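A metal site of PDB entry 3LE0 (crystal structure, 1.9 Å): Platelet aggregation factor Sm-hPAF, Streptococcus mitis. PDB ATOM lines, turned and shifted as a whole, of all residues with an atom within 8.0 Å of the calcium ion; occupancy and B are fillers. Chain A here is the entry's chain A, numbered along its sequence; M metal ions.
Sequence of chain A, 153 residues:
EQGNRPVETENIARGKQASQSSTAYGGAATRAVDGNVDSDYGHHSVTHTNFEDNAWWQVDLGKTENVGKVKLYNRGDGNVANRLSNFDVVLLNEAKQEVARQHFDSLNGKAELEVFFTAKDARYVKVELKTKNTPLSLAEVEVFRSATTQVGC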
ATOM      1  N   ALA A  28      20.157 -20.146  32.774  1.00  0.00           N
ATOM      2  CA  ALA A  28      19.556 -21.357  32.201  1.00  0.00           C
ATOM      3  C   ALA A  28      20.552 -22.520  32.036  1.00  0.00           C
ATOM      4  O   ALA A  28      21.684 -22.320  31.575  1.00  0.00           O
ATOM      5  CB  ALA A  28      18.896 -21.051  30.867  1.00  0.00           C
ATOM      6  N   ALA A  29      20.117 -23.720  32.419  1.00  0.00           N
ATOM      7  CA  ALA A  29      20.938 -24.938  32.291  1.00  0.00           C
ATOM      8  C   ALA A  29      21.523 -25.134  30.878  1.00  0.00           C
ATOM      9  O   ALA A  29      22.651 -25.624  30.752  1.00  0.00           O
ATOM     10  CB  ALA A  29      20.089 -26.176  32.669  1.00  0.00           C
ATOM     11  N   THR A  30      20.751 -24.796  29.847  1.00  0.00           N
ATOM     12  CA  THR A  30      21.213 -24.973  28.463  1.00  0.00           C
ATOM     13  C   THR A  30      22.446 -24.114  28.129  1.00  0.00           C
ATOM     14  O   THR A  30      23.114 -24.365  27.123  1.00  0.00           O
ATOM     15  CB  THR A  30      20.100 -24.660  27.451  1.00  0.00           C
ATOM     16  OG1 THR A  30      19.557 -23.384  27.761  1.00  0.00           O
ATOM     17  CG2 THR A  30      19.019 -25.649  27.563  1.00  0.00           C
ATOM     18  N   ARG A  31      22.776 -23.157  28.993  1.00  0.00           N
ATOM     19  CA  ARG A  31      23.969 -22.341  28.751  1.00  0.00           C
ATOM     20  C   ARG A  31      25.273 -23.112  28.842  1.00  0.00           C
ATOM     21  O   ARG A  31      26.273 -22.702  28.278  1.00  0.00           O
ATOM     22  CB  ARG A  31      24.043 -21.149  29.685  1.00  0.00           C
ATOM     23  CG  ARG A  31      22.973 -20.087  29.353  1.00  0.00           C
ATOM     24  CD  ARG A  31      22.984 -19.011  30.430  1.00  0.00           C
ATOM     25  NE  ARG A  31      21.974 -17.978  30.144  1.00  0.00           N
ATOM     26  CZ  ARG A  31      21.889 -16.821  30.788  1.00  0.00           C
ATOM     27  NH1 ARG A  31      20.964 -15.936  30.406  1.00  0.00           N
ATOM     28  NH2 ARG A  31      22.747 -16.534  31.783  1.00  0.00           N
ATOM     29  N   ALA A  32      25.265 -24.236  29.550  1.00  0.00           N
ATOM     30  CA  ALA A  32      26.472 -25.064  29.630  1.00  0.00           C
ATOM     31  C   ALA A  32      26.624 -25.977  28.382  1.00  0.00           C
ATOM     32  O   ALA A  32      27.639 -26.659  28.249  1.00  0.00           O
ATOM     33  CB  ALA A  32      26.502 -25.916  30.938  1.00  0.00           C
ATOM     34  N   VAL A  33      25.641 -25.993  27.489  1.00  0.00           N
ATOM     35  CA  VAL A  33      25.736 -26.839  26.267  1.00  0.00           C
ATOM     36  C   VAL A  33      25.452 -26.031  24.992  1.00  0.00           C
ATOM     37  O   VAL A  33      25.078 -26.576  23.973  1.00  0.00           O
ATOM     38  CB  VAL A  33      24.874 -28.151  26.344  1.00  0.00           C
ATOM     39  CG1 VAL A  33      25.439 -29.100  27.431  1.00  0.00           C
ATOM     40  CG2 VAL A  33      23.358 -27.859  26.512  1.00  0.00           C
ATOM     41  N   ASP A  34      25.687 -24.719  25.079  1.00  0.00           N
ATOM     42  CA  ASP A  34      25.423 -23.817  23.969  1.00  0.00           C
ATOM     43  C   ASP A  34      26.594 -23.605  23.004  1.00  0.00           C
ATOM     44  O   ASP A  34      26.491 -22.776  22.094  1.00  0.00           O
ATOM     45  CB  ASP A  34      24.872 -22.468  24.479  1.00  0.00           C
ATOM     46  CG  ASP A  34      25.888 -21.657  25.251  1.00  0.00           C
ATOM     47  OD1 ASP A  34      27.034 -22.092  25.547  1.00  0.00           O
ATOM     48  OD2 ASP A  34      25.507 -20.529  25.643  1.00  0.00           O
ATOM     49  N   GLY A  35      27.693 -24.324  23.224  1.00  0.00           N
ATOM     50  CA  GLY A  35      28.840 -24.215  22.336  1.00  0.00           C
ATOM     51  C   GLY A  35      29.652 -22.952  22.557  1.00  0.00           C
ATOM     52  O   GLY A  35      30.352 -22.489  21.675  1.00  0.00           O
ATOM     53  N   ASN A  36      29.531 -22.377  23.741  1.00  0.00           N
ATOM     54  CA  ASN A  36      30.244 -21.143  24.049  1.00  0.00           C
ATOM     55  C   ASN A  36      30.905 -21.277  25.418  1.00  0.00           C
ATOM     56  O   ASN A  36      30.238 -21.294  26.428  1.00  0.00           O
ATOM     57  CB  ASN A  36      29.246 -19.954  23.974  1.00  0.00           C
ATOM     58  CG  ASN A  36      29.930 -18.597  24.163  1.00  0.00           C
ATOM     59  OD1 ASN A  36      31.118 -18.543  24.497  1.00  0.00           O
ATOM     60  ND2 ASN A  36      29.178 -17.502  23.969  1.00  0.00           N
ATOM     61  N   VAL A  37      32.242 -21.386  25.468  1.00  0.00           N
ATOM     62  CA  VAL A  37      32.917 -21.543  26.736  1.00  0.00           C
ATOM     63  C   VAL A  37      33.176 -20.231  27.475  1.00  0.00           C
ATOM     64  O   VAL A  37      33.768 -20.253  28.553  1.00  0.00           O
ATOM     65  CB  VAL A  37      34.270 -22.324  26.593  1.00  0.00           C
ATOM     66  CG1 VAL A  37      34.006 -23.699  25.955  1.00  0.00           C
ATOM     67  CG2 VAL A  37      35.282 -21.527  25.772  1.00  0.00           C
ATOM     68  N   ASP A  38      32.747 -19.105  26.889  1.00  0.00           N
ATOM     69  CA  ASP A  38      32.954 -17.779  27.556  1.00  0.00           C
ATOM     70  C   ASP A  38      32.511 -17.805  29.056  1.00  0.00           C
ATOM     71  O   ASP A  38      31.340 -18.010  29.352  1.00  0.00           O
ATOM     72  CB  ASP A  38      32.178 -16.683  26.820  1.00  0.00           C
ATOM     73  CG  ASP A  38      32.550 -15.278  27.270  1.00  0.00           C
ATOM     74  OD1 ASP A  38      32.482 -14.376  26.410  1.00  0.00           O
ATOM     75  OD2 ASP A  38      32.886 -15.060  28.449  1.00  0.00           O
ATOM     76  N   SER A  39      33.454 -17.579  29.965  1.00  0.00           N
ATOM     77  CA  SER A  39      33.223 -17.810  31.381  1.00  0.00           C
ATOM     78  C   SER A  39      32.703 -16.600  32.176  1.00  0.00           C
ATOM     79  O   SER A  39      32.490 -16.676  33.387  1.00  0.00           O
ATOM     80  CB  SER A  39      34.507 -18.399  31.999  1.00  0.00           C
ATOM     81  OG  SER A  39      35.488 -17.390  32.129  1.00  0.00           O
ATOM     82  N   HIS A  43      28.225 -12.316  30.027  1.00  0.00           N
ATOM     83  CA  HIS A  43      28.081 -12.675  28.608  1.00  0.00           C
ATOM     84  C   HIS A  43      27.030 -13.764  28.331  1.00  0.00           C
ATOM     85  O   HIS A  43      26.894 -14.211  27.149  1.00  0.00           O
ATOM     86  CB  HIS A  43      29.434 -13.040  27.967  1.00  0.00           C
ATOM     87  CG  HIS A  43      30.463 -11.964  28.117  1.00  0.00           C
ATOM     88  ND1 HIS A  43      31.798 -12.154  27.838  1.00  0.00           N
ATOM     89  CD2 HIS A  43      30.341 -10.670  28.534  1.00  0.00           C
ATOM     90  CE1 HIS A  43      32.469 -11.030  28.069  1.00  0.00           C
ATOM     91  NE2 HIS A  43      31.596 -10.105  28.476  1.00  0.00           N
ATOM     92  N   HIS A  44      26.297 -14.134  29.391  1.00  0.00           N
ATOM     93  CA  HIS A  44      25.080 -14.964  29.281  1.00  0.00           C
ATOM     94  C   HIS A  44      25.315 -16.401  28.798  1.00  0.00           C
ATOM     95  O   HIS A  44      24.387 -17.057  28.302  1.00  0.00           O
ATOM     96  CB  HIS A  44      24.058 -14.286  28.323  1.00  0.00           C
ATOM     97  CG  HIS A  44      23.748 -12.868  28.662  1.00  0.00           C
ATOM     98  ND1 HIS A  44      23.345 -12.472  29.919  1.00  0.00           N
ATOM     99  CD2 HIS A  44      23.695 -11.761  27.887  1.00  0.00           C
ATOM    100  CE1 HIS A  44      23.099 -11.167  29.907  1.00  0.00           C
ATOM    101  NE2 HIS A  44      23.297 -10.718  28.684  1.00  0.00           N
ATOM    102  N   SER A  45      26.537 -16.913  28.950  1.00  0.00           N
ATOM    103  CA  SER A  45      26.784 -18.305  28.578  1.00  0.00           C
ATOM    104  C   SER A  45      27.162 -19.217  29.778  1.00  0.00           C
ATOM    105  O   SER A  45      27.736 -20.324  29.604  1.00  0.00           O
ATOM    106  CB  SER A  45      27.832 -18.417  27.460  1.00  0.00           C
ATOM    107  OG  SER A  45      27.693 -19.682  26.792  1.00  0.00           O
ATOM    108  N   VAL A  46      26.829 -18.766  30.980  1.00  0.00           N
ATOM    109  CA  VAL A  46      27.156 -19.507  32.206  1.00  0.00           C
ATOM    110  C   VAL A  46      25.834 -19.779  32.950  1.00  0.00           C
ATOM    111  O   VAL A  46      24.977 -18.885  33.090  1.00  0.00           O
ATOM    112  CB  VAL A  46      28.144 -18.688  33.088  1.00  0.00           C
ATOM    113  CG1 VAL A  46      28.536 -19.455  34.325  1.00  0.00           C
ATOM    114  CG2 VAL A  46      29.404 -18.243  32.280  1.00  0.00           C
ATOM    115  N   THR A  47      25.703 -20.998  33.476  1.00  0.00           N
ATOM    116  CA  THR A  47      24.512 -21.397  34.234  1.00  0.00           C
ATOM    117  C   THR A  47      24.577 -20.855  35.664  1.00  0.00           C
ATOM    118  O   THR A  47      25.634 -20.358  36.112  1.00  0.00           O
ATOM    119  CB  THR A  47      24.418 -22.940  34.329  1.00  0.00           C
ATOM    120  OG1 THR A  47      25.486 -23.400  35.171  1.00  0.00           O
ATOM    121  CG2 THR A  47      24.541 -23.578  32.940  1.00  0.00           C
ATOM    122  N   TYR A  73      33.996 -26.326  32.177  1.00  0.00           N
ATOM    123  CA  TYR A  73      34.549 -24.965  32.099  1.00  0.00           C
ATOM    124  C   TYR A  73      33.903 -24.168  33.193  1.00  0.00           C
ATOM    125  O   TYR A  73      32.666 -24.039  33.240  1.00  0.00           O
ATOM    126  CB  TYR A  73      34.266 -24.338  30.750  1.00  0.00           C
ATOM    127  CG  TYR A  73      34.971 -25.013  29.590  1.00  0.00           C
ATOM    128  CD1 TYR A  73      36.143 -24.463  29.036  1.00  0.00           C
ATOM    129  CD2 TYR A  73      34.470 -26.190  29.051  1.00  0.00           C
ATOM    130  CE1 TYR A  73      36.762 -25.081  27.953  1.00  0.00           C
ATOM    131  CE2 TYR A  73      35.105 -26.826  27.988  1.00  0.00           C
ATOM    132  CZ  TYR A  73      36.225 -26.267  27.443  1.00  0.00           C
ATOM    133  OH  TYR A  73      36.790 -26.931  26.374  1.00  0.00           O
ATOM    134  N   LEU A 138      28.240 -23.269  35.641  1.00  0.00           N
ATOM    135  CA  LEU A 138      29.160 -23.887  34.689  1.00  0.00           C
ATOM    136  C   LEU A 138      29.125 -23.043  33.408  1.00  0.00           C
ATOM    137  O   LEU A 138      28.026 -22.748  32.877  1.00  0.00           O
ATOM    138  CB  LEU A 138      28.683 -25.328  34.376  1.00  0.00           C
ATOM    139  CG  LEU A 138      28.783 -26.268  35.581  1.00  0.00           C
ATOM    140  CD1 LEU A 138      27.851 -27.481  35.340  1.00  0.00           C
ATOM    141  CD2 LEU A 138      30.267 -26.693  35.721  1.00  0.00           C
ATOM    142  N   ALA A 139      30.304 -22.681  32.905  1.00  0.00           N
ATOM    143  CA  ALA A 139      30.368 -21.974  31.622  1.00  0.00           C
ATOM    144  C   ALA A 139      30.061 -22.940  30.469  1.00  0.00           C
ATOM    145  O   ALA A 139      29.444 -22.582  29.500  1.00  0.00           O
ATOM    146  CB  ALA A 139      31.774 -21.312  31.439  1.00  0.00           C
ATOM    147  N   GLU A 140      30.497 -24.197  30.593  1.00  0.00           N
ATOM    148  CA  GLU A 140      30.246 -25.186  29.562  1.00  0.00           C
ATOM    149  C   GLU A 140      30.622 -26.557  30.120  1.00  0.00           C
ATOM    150  O   GLU A 140      31.493 -26.659  30.990  1.00  0.00           O
ATOM    151  CB  GLU A 140      31.101 -24.897  28.290  1.00  0.00           C
ATOM    152  CG  GLU A 140      30.680 -25.704  27.037  1.00  0.00           C
ATOM    153  CD  GLU A 140      29.474 -25.100  26.295  1.00  0.00           C
ATOM    154  OE1 GLU A 140      28.878 -24.114  26.803  1.00  0.00           O
ATOM    155  OE2 GLU A 140      29.085 -25.636  25.238  1.00  0.00           O
ATOM    156  N   VAL A 141      29.912 -27.572  29.609  1.00  0.00           N
ATOM    157  CA  VAL A 141      30.266 -28.987  29.830  1.00  0.00           C
ATOM    158  C   VAL A 141      30.299 -29.643  28.466  1.00  0.00           C
ATOM    159  O   VAL A 141      29.293 -29.624  27.714  1.00  0.00           O
ATOM    160  CB  VAL A 141      29.240 -29.724  30.757  1.00  0.00           C
ATOM    161  CG1 VAL A 141      29.631 -31.219  30.916  1.00  0.00           C
ATOM    162  CG2 VAL A 141      29.143 -29.029  32.137  1.00  0.00           C
HETATM  163 CA    CA M   1      28.272 -21.845  27.617  1.00  0.00          CA
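NH2 of Arg 31 sits close to O of Val 46 (3.5 Å).
NE of Arg 31 lies within hydrogen-bond range of O of His 44 (3.2 Å).
The backbone NH (N) of Ala 139 is in hydrogen-bond range of the backbone carbonyl oxygen (O) of Tyr 73, at 2.7 Å.
The side-chain amide oxygen (OD1) of Asn 36 lies within hydrogen-bond range of the backbone NH (N) of Asp 38.
OE2 of Glu 140 lies within hydrogen-bond range of N of Gly 35.
The backbone carbonyl oxygen (O) of Glu 140 sits at hydrogen-bond distance from the backbone NH (N) of Tyr 73, 2.8 Å away.
O of Arg 31 binds the calcium ion (2.3 Å).
The calcium ion is bound by the backbone carbonyl oxygen (O) of Ala 139, 2.3 Å away.
The backbone carbonyl oxygen (O) of Asn 36 binds the calcium ion, 2.4 Å away.
The side-chain hydroxyl (OG) of Ser 45 is bound to the calcium ion (2.4 Å).
OD1 of Asp 34 binds the calcium ion (2.4 Å).
The side-chain carboxylate (OE1) of Glu 140 binds the calcium ion, at 2.5 Å.
The calcium ion is bound by the backbone carbonyl oxygen (O) of Ser 45, 2.6 Å away.
The calcium ion has seven donor atoms within binding distance.
Six residues have an atom within 4 Å of the calcium ion: Arg 31, Asp 34, Asn 36, Ser 45, Ala 139 and Glu 140.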
